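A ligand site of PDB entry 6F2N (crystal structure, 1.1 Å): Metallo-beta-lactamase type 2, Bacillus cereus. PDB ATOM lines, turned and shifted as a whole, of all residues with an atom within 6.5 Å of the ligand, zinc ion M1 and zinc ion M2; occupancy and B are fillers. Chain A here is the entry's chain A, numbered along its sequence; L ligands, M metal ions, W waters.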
ATOM      1  N   VAL A  39      24.814  27.388  13.625  1.00  0.00           N
ATOM      2  CA  VAL A  39      25.439  28.145  12.545  1.00  0.00           C
ATOM      3  C   VAL A  39      24.301  28.891  11.875  1.00  0.00           C
ATOM      4  O   VAL A  39      23.453  28.245  11.225  1.00  0.00           O
ATOM      5  CB  VAL A  39      26.170  27.231  11.537  1.00  0.00           C
ATOM      6  CG1 VAL A  39      26.783  28.088  10.372  1.00  0.00           C
ATOM      7  CG2 VAL A  39      27.243  26.385  12.207  1.00  0.00           C
ATOM      8  N   PRO A  40      24.258  30.222  11.958  1.00  0.00           N
ATOM      9  CA  PRO A  40      23.224  30.971  11.231  1.00  0.00           C
ATOM     10  C   PRO A  40      23.534  31.108   9.773  1.00  0.00           C
ATOM     11  O   PRO A  40      24.686  31.082   9.361  1.00  0.00           O
ATOM     12  CB  PRO A  40      23.270  32.346  11.892  1.00  0.00           C
ATOM     13  CG  PRO A  40      24.660  32.515  12.147  1.00  0.00           C
ATOM     14  CD  PRO A  40      25.133  31.142  12.665  1.00  0.00           C
ATOM     15  N   SER A  41      22.471  31.267   8.987  1.00  0.00           N
ATOM     16  CA  SER A  41      22.634  31.534   7.583  1.00  0.00           C
ATOM     17  C   SER A  41      21.534  32.454   7.107  1.00  0.00           C
ATOM     18  O   SER A  41      20.448  32.499   7.701  1.00  0.00           O
ATOM     19  CB  SER A  41      22.604  30.242   6.781  1.00  0.00           C
ATOM     20  OG  SER A  41      21.365  29.590   6.987  1.00  0.00           O
ATOM     21  N   TRP A  59      18.870  24.915   5.645  1.00  0.00           N
ATOM     22  CA  TRP A  59      19.735  23.769   5.895  1.00  0.00           C
ATOM     23  C   TRP A  59      19.089  22.440   5.626  1.00  0.00           C
ATOM     24  O   TRP A  59      19.824  21.475   5.359  1.00  0.00           O
ATOM     25  CB  TRP A  59      20.207  23.807   7.355  1.00  0.00           C
ATOM     26  CG  TRP A  59      20.995  24.988   7.725  1.00  0.00           C
ATOM     27  CD1 TRP A  59      20.521  26.192   8.240  1.00  0.00           C
ATOM     28  CD2 TRP A  59      22.416  25.127   7.601  1.00  0.00           C
ATOM     29  NE1 TRP A  59      21.613  27.033   8.502  1.00  0.00           N
ATOM     30  CE2 TRP A  59      22.771  26.401   8.118  1.00  0.00           C
ATOM     31  CE3 TRP A  59      23.461  24.245   7.173  1.00  0.00           C
ATOM     32  CZ2 TRP A  59      24.097  26.839   8.210  1.00  0.00           C
ATOM     33  CZ3 TRP A  59      24.756  24.706   7.248  1.00  0.00           C
ATOM     34  CH2 TRP A  59      25.076  25.968   7.809  1.00  0.00           C
ATOM     35  N   HIS A  86      24.156  28.214  -4.532  1.00  0.00           N
ATOM     36  CA  HIS A  86      25.176  27.178  -4.761  1.00  0.00           C
ATOM     37  C   HIS A  86      24.633  25.889  -4.142  1.00  0.00           C
ATOM     38  O   HIS A  86      23.575  25.851  -3.554  1.00  0.00           O
ATOM     39  CB  HIS A  86      26.594  27.522  -4.309  1.00  0.00           C
ATOM     40  CG  HIS A  86      26.811  27.640  -2.844  1.00  0.00           C
ATOM     41  ND1 HIS A  86      26.548  28.791  -2.141  1.00  0.00           N
ATOM     42  CD2 HIS A  86      27.445  26.818  -1.956  1.00  0.00           C
ATOM     43  CE1 HIS A  86      26.898  28.584  -0.890  1.00  0.00           C
ATOM     44  NE2 HIS A  86      27.478  27.431  -0.743  1.00  0.00           N
ATOM     45  N   ALA A  87      25.364  24.804  -4.341  1.00  0.00           N
ATOM     46  CA  ALA A  87      24.899  23.437  -4.027  1.00  0.00           C
ATOM     47  C   ALA A  87      25.300  22.902  -2.649  1.00  0.00           C
ATOM     48  O   ALA A  87      24.982  21.720  -2.401  1.00  0.00           O
ATOM     49  CB  ALA A  87      25.288  22.459  -5.130  1.00  0.00           C
ATOM     50  N   HIS A  88      25.610  23.720  -1.702  1.00  0.00           N
ATOM     51  CA  HIS A  88      25.814  23.289  -0.303  1.00  0.00           C
ATOM     52  C   HIS A  88      24.448  23.285   0.479  1.00  0.00           C
ATOM     53  O   HIS A  88      23.515  23.958   0.151  1.00  0.00           O
ATOM     54  CB  HIS A  88      26.799  24.221   0.434  1.00  0.00           C
ATOM     55  CG  HIS A  88      28.258  24.031   0.085  1.00  0.00           C
ATOM     56  ND1 HIS A  88      29.198  25.007   0.313  1.00  0.00           N
ATOM     57  CD2 HIS A  88      28.932  22.959  -0.385  1.00  0.00           C
ATOM     58  CE1 HIS A  88      30.398  24.548  -0.021  1.00  0.00           C
ATOM     59  NE2 HIS A  88      30.260  23.296  -0.429  1.00  0.00           N
ATOM     60  N   ALA A  89      24.455  22.583   1.614  1.00  0.00           N
ATOM     61  CA  ALA A  89      23.228  22.341   2.381  1.00  0.00           C
ATOM     62  C   ALA A  89      22.533  23.618   2.867  1.00  0.00           C
ATOM     63  O   ALA A  89      21.291  23.647   2.950  1.00  0.00           O
ATOM     64  CB  ALA A  89      23.505  21.441   3.568  1.00  0.00           C
ATOM     65  N   ASP A  90      23.267  24.618   3.299  1.00  0.00           N
ATOM     66  CA  ASP A  90      22.679  25.854   3.783  1.00  0.00           C
ATOM     67  C   ASP A  90      21.808  26.479   2.747  1.00  0.00           C
ATOM     68  O   ASP A  90      20.854  27.175   3.079  1.00  0.00           O
ATOM     69  CB  ASP A  90      23.675  26.854   4.367  1.00  0.00           C
ATOM     70  CG  ASP A  90      24.752  27.321   3.392  1.00  0.00           C
ATOM     71  OD1 ASP A  90      25.154  26.582   2.475  1.00  0.00           O
ATOM     72  OD2 ASP A  90      25.280  28.437   3.622  1.00  0.00           O
ATOM     73  N   ARG A  91      22.194  26.333   1.465  1.00  0.00           N
ATOM     74  CA  ARG A  91      21.425  26.890   0.365  1.00  0.00           C
ATOM     75  C   ARG A  91      20.339  25.999  -0.226  1.00  0.00           C
ATOM     76  O   ARG A  91      19.254  26.459  -0.564  1.00  0.00           O
ATOM     77  CB  ARG A  91      22.363  27.201  -0.809  1.00  0.00           C
ATOM     78  CG  ARG A  91      23.649  27.935  -0.467  1.00  0.00           C
ATOM     79  CD  ARG A  91      23.400  29.379  -0.080  1.00  0.00           C
ATOM     80  NE  ARG A  91      23.613  29.594   1.349  1.00  0.00           N
ATOM     81  CZ  ARG A  91      23.210  30.664   2.021  1.00  0.00           C
ATOM     82  NH1 ARG A  91      22.540  31.626   1.394  1.00  0.00           N
ATOM     83  NH2 ARG A  91      23.457  30.768   3.316  1.00  0.00           N
ATOM     84  N   HIS A 149      33.950  30.805  -3.220  1.00  0.00           N
ATOM     85  CA  HIS A 149      33.588  29.926  -2.129  1.00  0.00           C
ATOM     86  C   HIS A 149      33.333  28.515  -2.610  1.00  0.00           C
ATOM     87  O   HIS A 149      33.689  27.542  -1.959  1.00  0.00           O
ATOM     88  CB  HIS A 149      32.381  30.506  -1.407  1.00  0.00           C
ATOM     89  CG  HIS A 149      31.708  29.549  -0.503  1.00  0.00           C
ATOM     90  ND1 HIS A 149      32.240  29.139   0.709  1.00  0.00           N
ATOM     91  CD2 HIS A 149      30.565  28.876  -0.661  1.00  0.00           C
ATOM     92  CE1 HIS A 149      31.394  28.279   1.262  1.00  0.00           C
ATOM     93  NE2 HIS A 149      30.339  28.082   0.440  1.00  0.00           N
ATOM     94  N   THR A 150      32.652  28.392  -3.748  1.00  0.00           N
ATOM     95  CA  THR A 150      32.487  27.178  -4.502  1.00  0.00           C
ATOM     96  C   THR A 150      32.725  27.473  -5.967  1.00  0.00           C
ATOM     97  O   THR A 150      32.780  28.615  -6.400  1.00  0.00           O
ATOM     98  CB  THR A 150      31.134  26.523  -4.303  1.00  0.00           C
ATOM     99  OG1 THR A 150      30.150  27.471  -4.724  1.00  0.00           O
ATOM    100  CG2 THR A 150      30.929  26.063  -2.874  1.00  0.00           C
ATOM    101  N   GLY A 167      25.677  36.030  -0.910  1.00  0.00           N
ATOM    102  CA  GLY A 167      25.764  34.657  -0.600  1.00  0.00           C
ATOM    103  C   GLY A 167      27.104  34.321   0.033  1.00  0.00           C
ATOM    104  O   GLY A 167      27.788  35.169   0.589  1.00  0.00           O
ATOM    105  N   CYS A 168      27.499  33.061  -0.079  1.00  0.00           N
ATOM    106  CA  CYS A 168      28.635  32.615   0.645  1.00  0.00           C
ATOM    107  C   CYS A 168      29.963  32.995  -0.002  1.00  0.00           C
ATOM    108  O   CYS A 168      31.002  32.859   0.635  1.00  0.00           O
ATOM    109  CB  CYS A 168      28.496  31.161   0.955  1.00  0.00           C
ATOM    110  SG  CYS A 168      26.842  30.801   1.771  1.00  0.00           S
ATOM    111  N   LEU A 169      29.901  33.577  -1.181  1.00  0.00           N
ATOM    112  CA  LEU A 169      31.054  34.275  -1.786  1.00  0.00           C
ATOM    113  C   LEU A 169      31.517  35.444  -0.934  1.00  0.00           C
ATOM    114  O   LEU A 169      32.704  35.857  -1.023  1.00  0.00           O
ATOM    115  CB  LEU A 169      30.600  34.802  -3.168  1.00  0.00           C
ATOM    116  CG  LEU A 169      31.644  35.458  -4.008  1.00  0.00           C
ATOM    117  CD1 LEU A 169      32.661  34.460  -4.622  1.00  0.00           C
ATOM    118  CD2 LEU A 169      30.978  36.241  -5.161  1.00  0.00           C
ATOM    119  N   LYS A 171      31.987  37.290   2.763  1.00  0.00           N
ATOM    120  CA  LYS A 171      32.085  37.097   4.198  1.00  0.00           C
ATOM    121  C   LYS A 171      31.630  38.320   4.975  1.00  0.00           C
ATOM    122  O   LYS A 171      31.860  39.458   4.552  1.00  0.00           O
ATOM    123  CB  LYS A 171      33.558  36.791   4.521  1.00  0.00           C
ATOM    124  CG  LYS A 171      34.065  35.508   3.848  1.00  0.00           C
ATOM    125  CD  LYS A 171      33.321  34.264   4.399  1.00  0.00           C
ATOM    126  CE  LYS A 171      33.773  32.955   3.955  1.00  0.00           C
ATOM    127  NZ  LYS A 171      33.097  31.829   4.679  1.00  0.00           N
ATOM    128  N   LEU A 178      38.280  32.395   6.076  1.00  0.00           N
ATOM    129  CA  LEU A 178      37.426  32.022   4.963  1.00  0.00           C
ATOM    130  C   LEU A 178      36.487  30.874   5.269  1.00  0.00           C
ATOM    131  O   LEU A 178      35.678  30.541   4.434  1.00  0.00           O
ATOM    132  CB  LEU A 178      38.303  31.653   3.787  1.00  0.00           C
ATOM    133  CG  LEU A 178      39.188  32.802   3.238  1.00  0.00           C
ATOM    134  CD1 LEU A 178      40.226  32.253   2.292  1.00  0.00           C
ATOM    135  CD2 LEU A 178      38.278  33.865   2.570  1.00  0.00           C
ATOM    136  N   GLY A 179      36.609  30.253   6.412  1.00  0.00           N
ATOM    137  CA  GLY A 179      35.725  29.179   6.737  1.00  0.00           C
ATOM    138  C   GLY A 179      36.066  27.888   6.002  1.00  0.00           C
ATOM    139  O   GLY A 179      37.222  27.574   5.714  1.00  0.00           O
ATOM    140  N   ASN A 180      35.050  27.128   5.647  1.00  0.00           N
ATOM    141  CA  ASN A 180      35.254  25.841   5.003  1.00  0.00           C
ATOM    142  C   ASN A 180      35.619  26.086   3.540  1.00  0.00           C
ATOM    143  O   ASN A 180      34.793  26.567   2.746  1.00  0.00           O
ATOM    144  CB  ASN A 180      34.038  24.927   5.132  1.00  0.00           C
ATOM    145  CG  ASN A 180      34.330  23.493   4.686  1.00  0.00           C
ATOM    146  OD1 ASN A 180      34.939  23.279   3.671  1.00  0.00           O
ATOM    147  ND2 ASN A 180      33.834  22.502   5.458  1.00  0.00           N
ATOM    148  N   VAL A 181      36.838  25.715   3.187  1.00  0.00           N
ATOM    149  CA  VAL A 181      37.423  25.944   1.878  1.00  0.00           C
ATOM    150  C   VAL A 181      37.636  24.630   1.133  1.00  0.00           C
ATOM    151  O   VAL A 181      38.253  24.631   0.062  1.00  0.00           O
ATOM    152  CB  VAL A 181      38.694  26.806   1.923  1.00  0.00           C
ATOM    153  CG1 VAL A 181      38.433  28.217   2.387  1.00  0.00           C
ATOM    154  CG2 VAL A 181      39.803  26.087   2.813  1.00  0.00           C
ATOM    155  N   ALA A 182      36.990  23.558   1.587  1.00  0.00           N
ATOM    156  CA  ALA A 182      37.149  22.279   0.914  1.00  0.00           C
ATOM    157  C   ALA A 182      36.742  22.374  -0.569  1.00  0.00           C
ATOM    158  O   ALA A 182      37.336  21.704  -1.442  1.00  0.00           O
ATOM    159  CB  ALA A 182      36.266  21.214   1.586  1.00  0.00           C
ATOM    160  N   ASP A 183      35.706  23.135  -0.855  1.00  0.00           N
ATOM    161  CA  ASP A 183      35.153  23.235  -2.182  1.00  0.00           C
ATOM    162  C   ASP A 183      35.495  24.548  -2.857  1.00  0.00           C
ATOM    163  O   ASP A 183      34.918  24.866  -3.909  1.00  0.00           O
ATOM    164  CB  ASP A 183      33.635  22.992  -2.124  1.00  0.00           C
ATOM    165  CG  ASP A 183      33.290  21.602  -1.643  1.00  0.00           C
ATOM    166  OD1 ASP A 183      33.979  20.647  -2.004  1.00  0.00           O
ATOM    167  OD2 ASP A 183      32.292  21.490  -0.952  1.00  0.00           O
ATOM    168  N   GLY A 209      26.276  35.420   3.052  1.00  0.00           N
ATOM    169  CA  GLY A 209      25.615  34.146   3.287  1.00  0.00           C
ATOM    170  C   GLY A 209      25.414  33.832   4.746  1.00  0.00           C
ATOM    171  O   GLY A 209      24.474  33.114   5.124  1.00  0.00           O
ATOM    172  N   HIS A 210      26.303  34.358   5.594  1.00  0.00           N
ATOM    173  CA  HIS A 210      26.271  34.187   7.030  1.00  0.00           C
ATOM    174  C   HIS A 210      26.677  35.519   7.670  1.00  0.00           C
ATOM    175  O   HIS A 210      27.612  36.170   7.197  1.00  0.00           O
ATOM    176  CB  HIS A 210      27.239  33.014   7.473  1.00  0.00           C
ATOM    177  CG  HIS A 210      27.039  31.695   6.714  1.00  0.00           C
ATOM    178  ND1 HIS A 210      26.173  30.697   7.087  1.00  0.00           N
ATOM    179  CD2 HIS A 210      27.587  31.255   5.527  1.00  0.00           C
ATOM    180  CE1 HIS A 210      26.159  29.742   6.174  1.00  0.00           C
ATOM    181  NE2 HIS A 210      27.031  30.040   5.217  1.00  0.00           N
HETATM  182  C1  LIG L   1      31.124  24.194   3.259  1.00  0.00           C
HETATM  183  C2  LIG L   1      30.884  22.865   3.028  1.00  0.00           C
HETATM  184  C3  LIG L   1      29.834  22.248   3.628  1.00  0.00           C
HETATM  185  C4  LIG L   1      29.007  22.951   4.492  1.00  0.00           C
HETATM  186  C5  LIG L   1      29.204  24.309   4.750  1.00  0.00           C
HETATM  187  C6  LIG L   1      28.300  25.040   5.734  1.00  0.00           C
HETATM  188  C7  LIG L   1      29.012  25.748   6.888  1.00  0.00           C
HETATM  189  C8  LIG L   1      28.884  27.098   7.058  1.00  0.00           C
HETATM  190  C9  LIG L   1      29.524  27.789   8.112  1.00  0.00           C
HETATM  191  C10 LIG L   1      29.380  29.188   8.323  1.00  0.00           C
HETATM  192  C11 LIG L   1      30.029  29.818   9.352  1.00  0.00           C
HETATM  193  C12 LIG L   1      30.817  29.086  10.239  1.00  0.00           C
HETATM  194  C13 LIG L   1      29.631  27.407   3.797  1.00  0.00           C
HETATM  195  O1  LIG L   1      29.396  29.694   3.581  1.00  0.00           O
HETATM  196  C14 LIG L   1      30.100  28.785   4.066  1.00  0.00           C
HETATM  197  C15 LIG L   1      30.967  27.728  10.088  1.00  0.00           C
HETATM  198  C16 LIG L   1      30.326  27.050   9.019  1.00  0.00           C
HETATM  199  C17 LIG L   1      30.453  25.655   8.825  1.00  0.00           C
HETATM  200  C18 LIG L   1      29.804  25.037   7.780  1.00  0.00           C
HETATM  201  C19 LIG L   1      30.461  26.396   4.202  1.00  0.00           C
HETATM  202  C20 LIG L   1      30.276  24.945   4.086  1.00  0.00           C
HETATM  203  O2  LIG L   1      31.233  29.074   4.569  1.00  0.00           O
HETATM  204  S1  LIG L   1      28.086  27.092   3.013  1.00  0.00           S
HETATM  205 ZN    ZN M   1      27.243  29.235   3.345  1.00  0.00          ZN
HETATM  206 ZN    ZN M   2      28.747  26.899   0.787  1.00  0.00          ZN
HETATM  207  O   HOH W   1      27.428  31.301  10.661  1.00  0.00           O
HETATM  208  O   HOH W   2      32.503  28.337   6.658  1.00  0.00           O
HETATM  209  O   HOH W   3      30.635  32.160   3.336  1.00  0.00           O
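The side-chain amino group (NZ) of Lys 171 is in salt-bridge range of an oxygen (O2) of the ligand.
A ring nitrogen (NE2) of His 88 lies within hydrogen-bond range of the side-chain carboxylate (OD2) of Asp 183 (2.8 Å).
ND1 of His 210 lies within hydrogen-bond range of O of Pro 40.
The side-chain carboxylate (OD1) of Asp 90 is in salt-bridge range of the guanidinium group (NE) of Arg 91 (3.6 Å).
The side-chain sulfur (SG) of Cys 168 lies close to the guanidinium group (NE) of Arg 91, 3.5 Å away.
NZ of Lys 171 lies within hydrogen-bond range of O of Leu 178, 2.9 Å away.
The backbone NH of Ala 182 sits at hydrogen-bond distance from the side-chain amide oxygen of Asn 180 (2.9 Å).
The indole nitrogen of Trp 59 is in hydrogen-bond range of the side-chain hydroxyl of Ser 41 (3.0 Å).
Val 39 touches the ligand (CG1 to C10, 3.5 Å).
Trp 59 touches the ligand (CZ3 to C6, 3.9 Å).
Asn 180 touches the ligand.
Ten residues have an atom within 4 Å of the ligand: Val 39, Trp 59, His 86, His 88, Asp 90, His 149, Cys 168, Lys 171, Asn 180 and His 210.
Along chain A the residues within 4 Å of the ligand span positions 39 to 210.
The nearest printed residue that does not touch zinc ion M1 is Arg 91 (4.1 Å).
Within 4 Å of zinc ion M2: His 86, His 88, Asp 90 and His 149.
The nearest printed residue that does not touch zinc ion M2 is Cys 168 (4.3 Å).
Zinc ion M1 is bound by NE2 of His 210 (2.0 Å), OD2 of Asp 90 (2.1 Å), O1 of the ligand (2.2 Å), SG of Cys 168 (2.3 Å) and S1 of the ligand (2.3 Å).
Zinc ion M2 is bound by a ring nitrogen (ND1) of His 88 (2.0 Å), a ring nitrogen (NE2) of His 149 (2.0 Å), a ring nitrogen (NE2) of His 86 (2.1 Å) and a sulfur (S1) of the ligand (2.3 Å).
Zinc ion M2 has four donor atoms within binding distance.
Water W2 bridges an oxygen (O2) of the ligand (2.6 Å) and the backbone NH of Asn 180 (3.0 Å).
Water W3 lies within hydrogen-bond range of O of Cys 168 (2.8 Å), NZ of Lys 171 (2.8 Å) and O2 of the ligand (3.4 Å).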
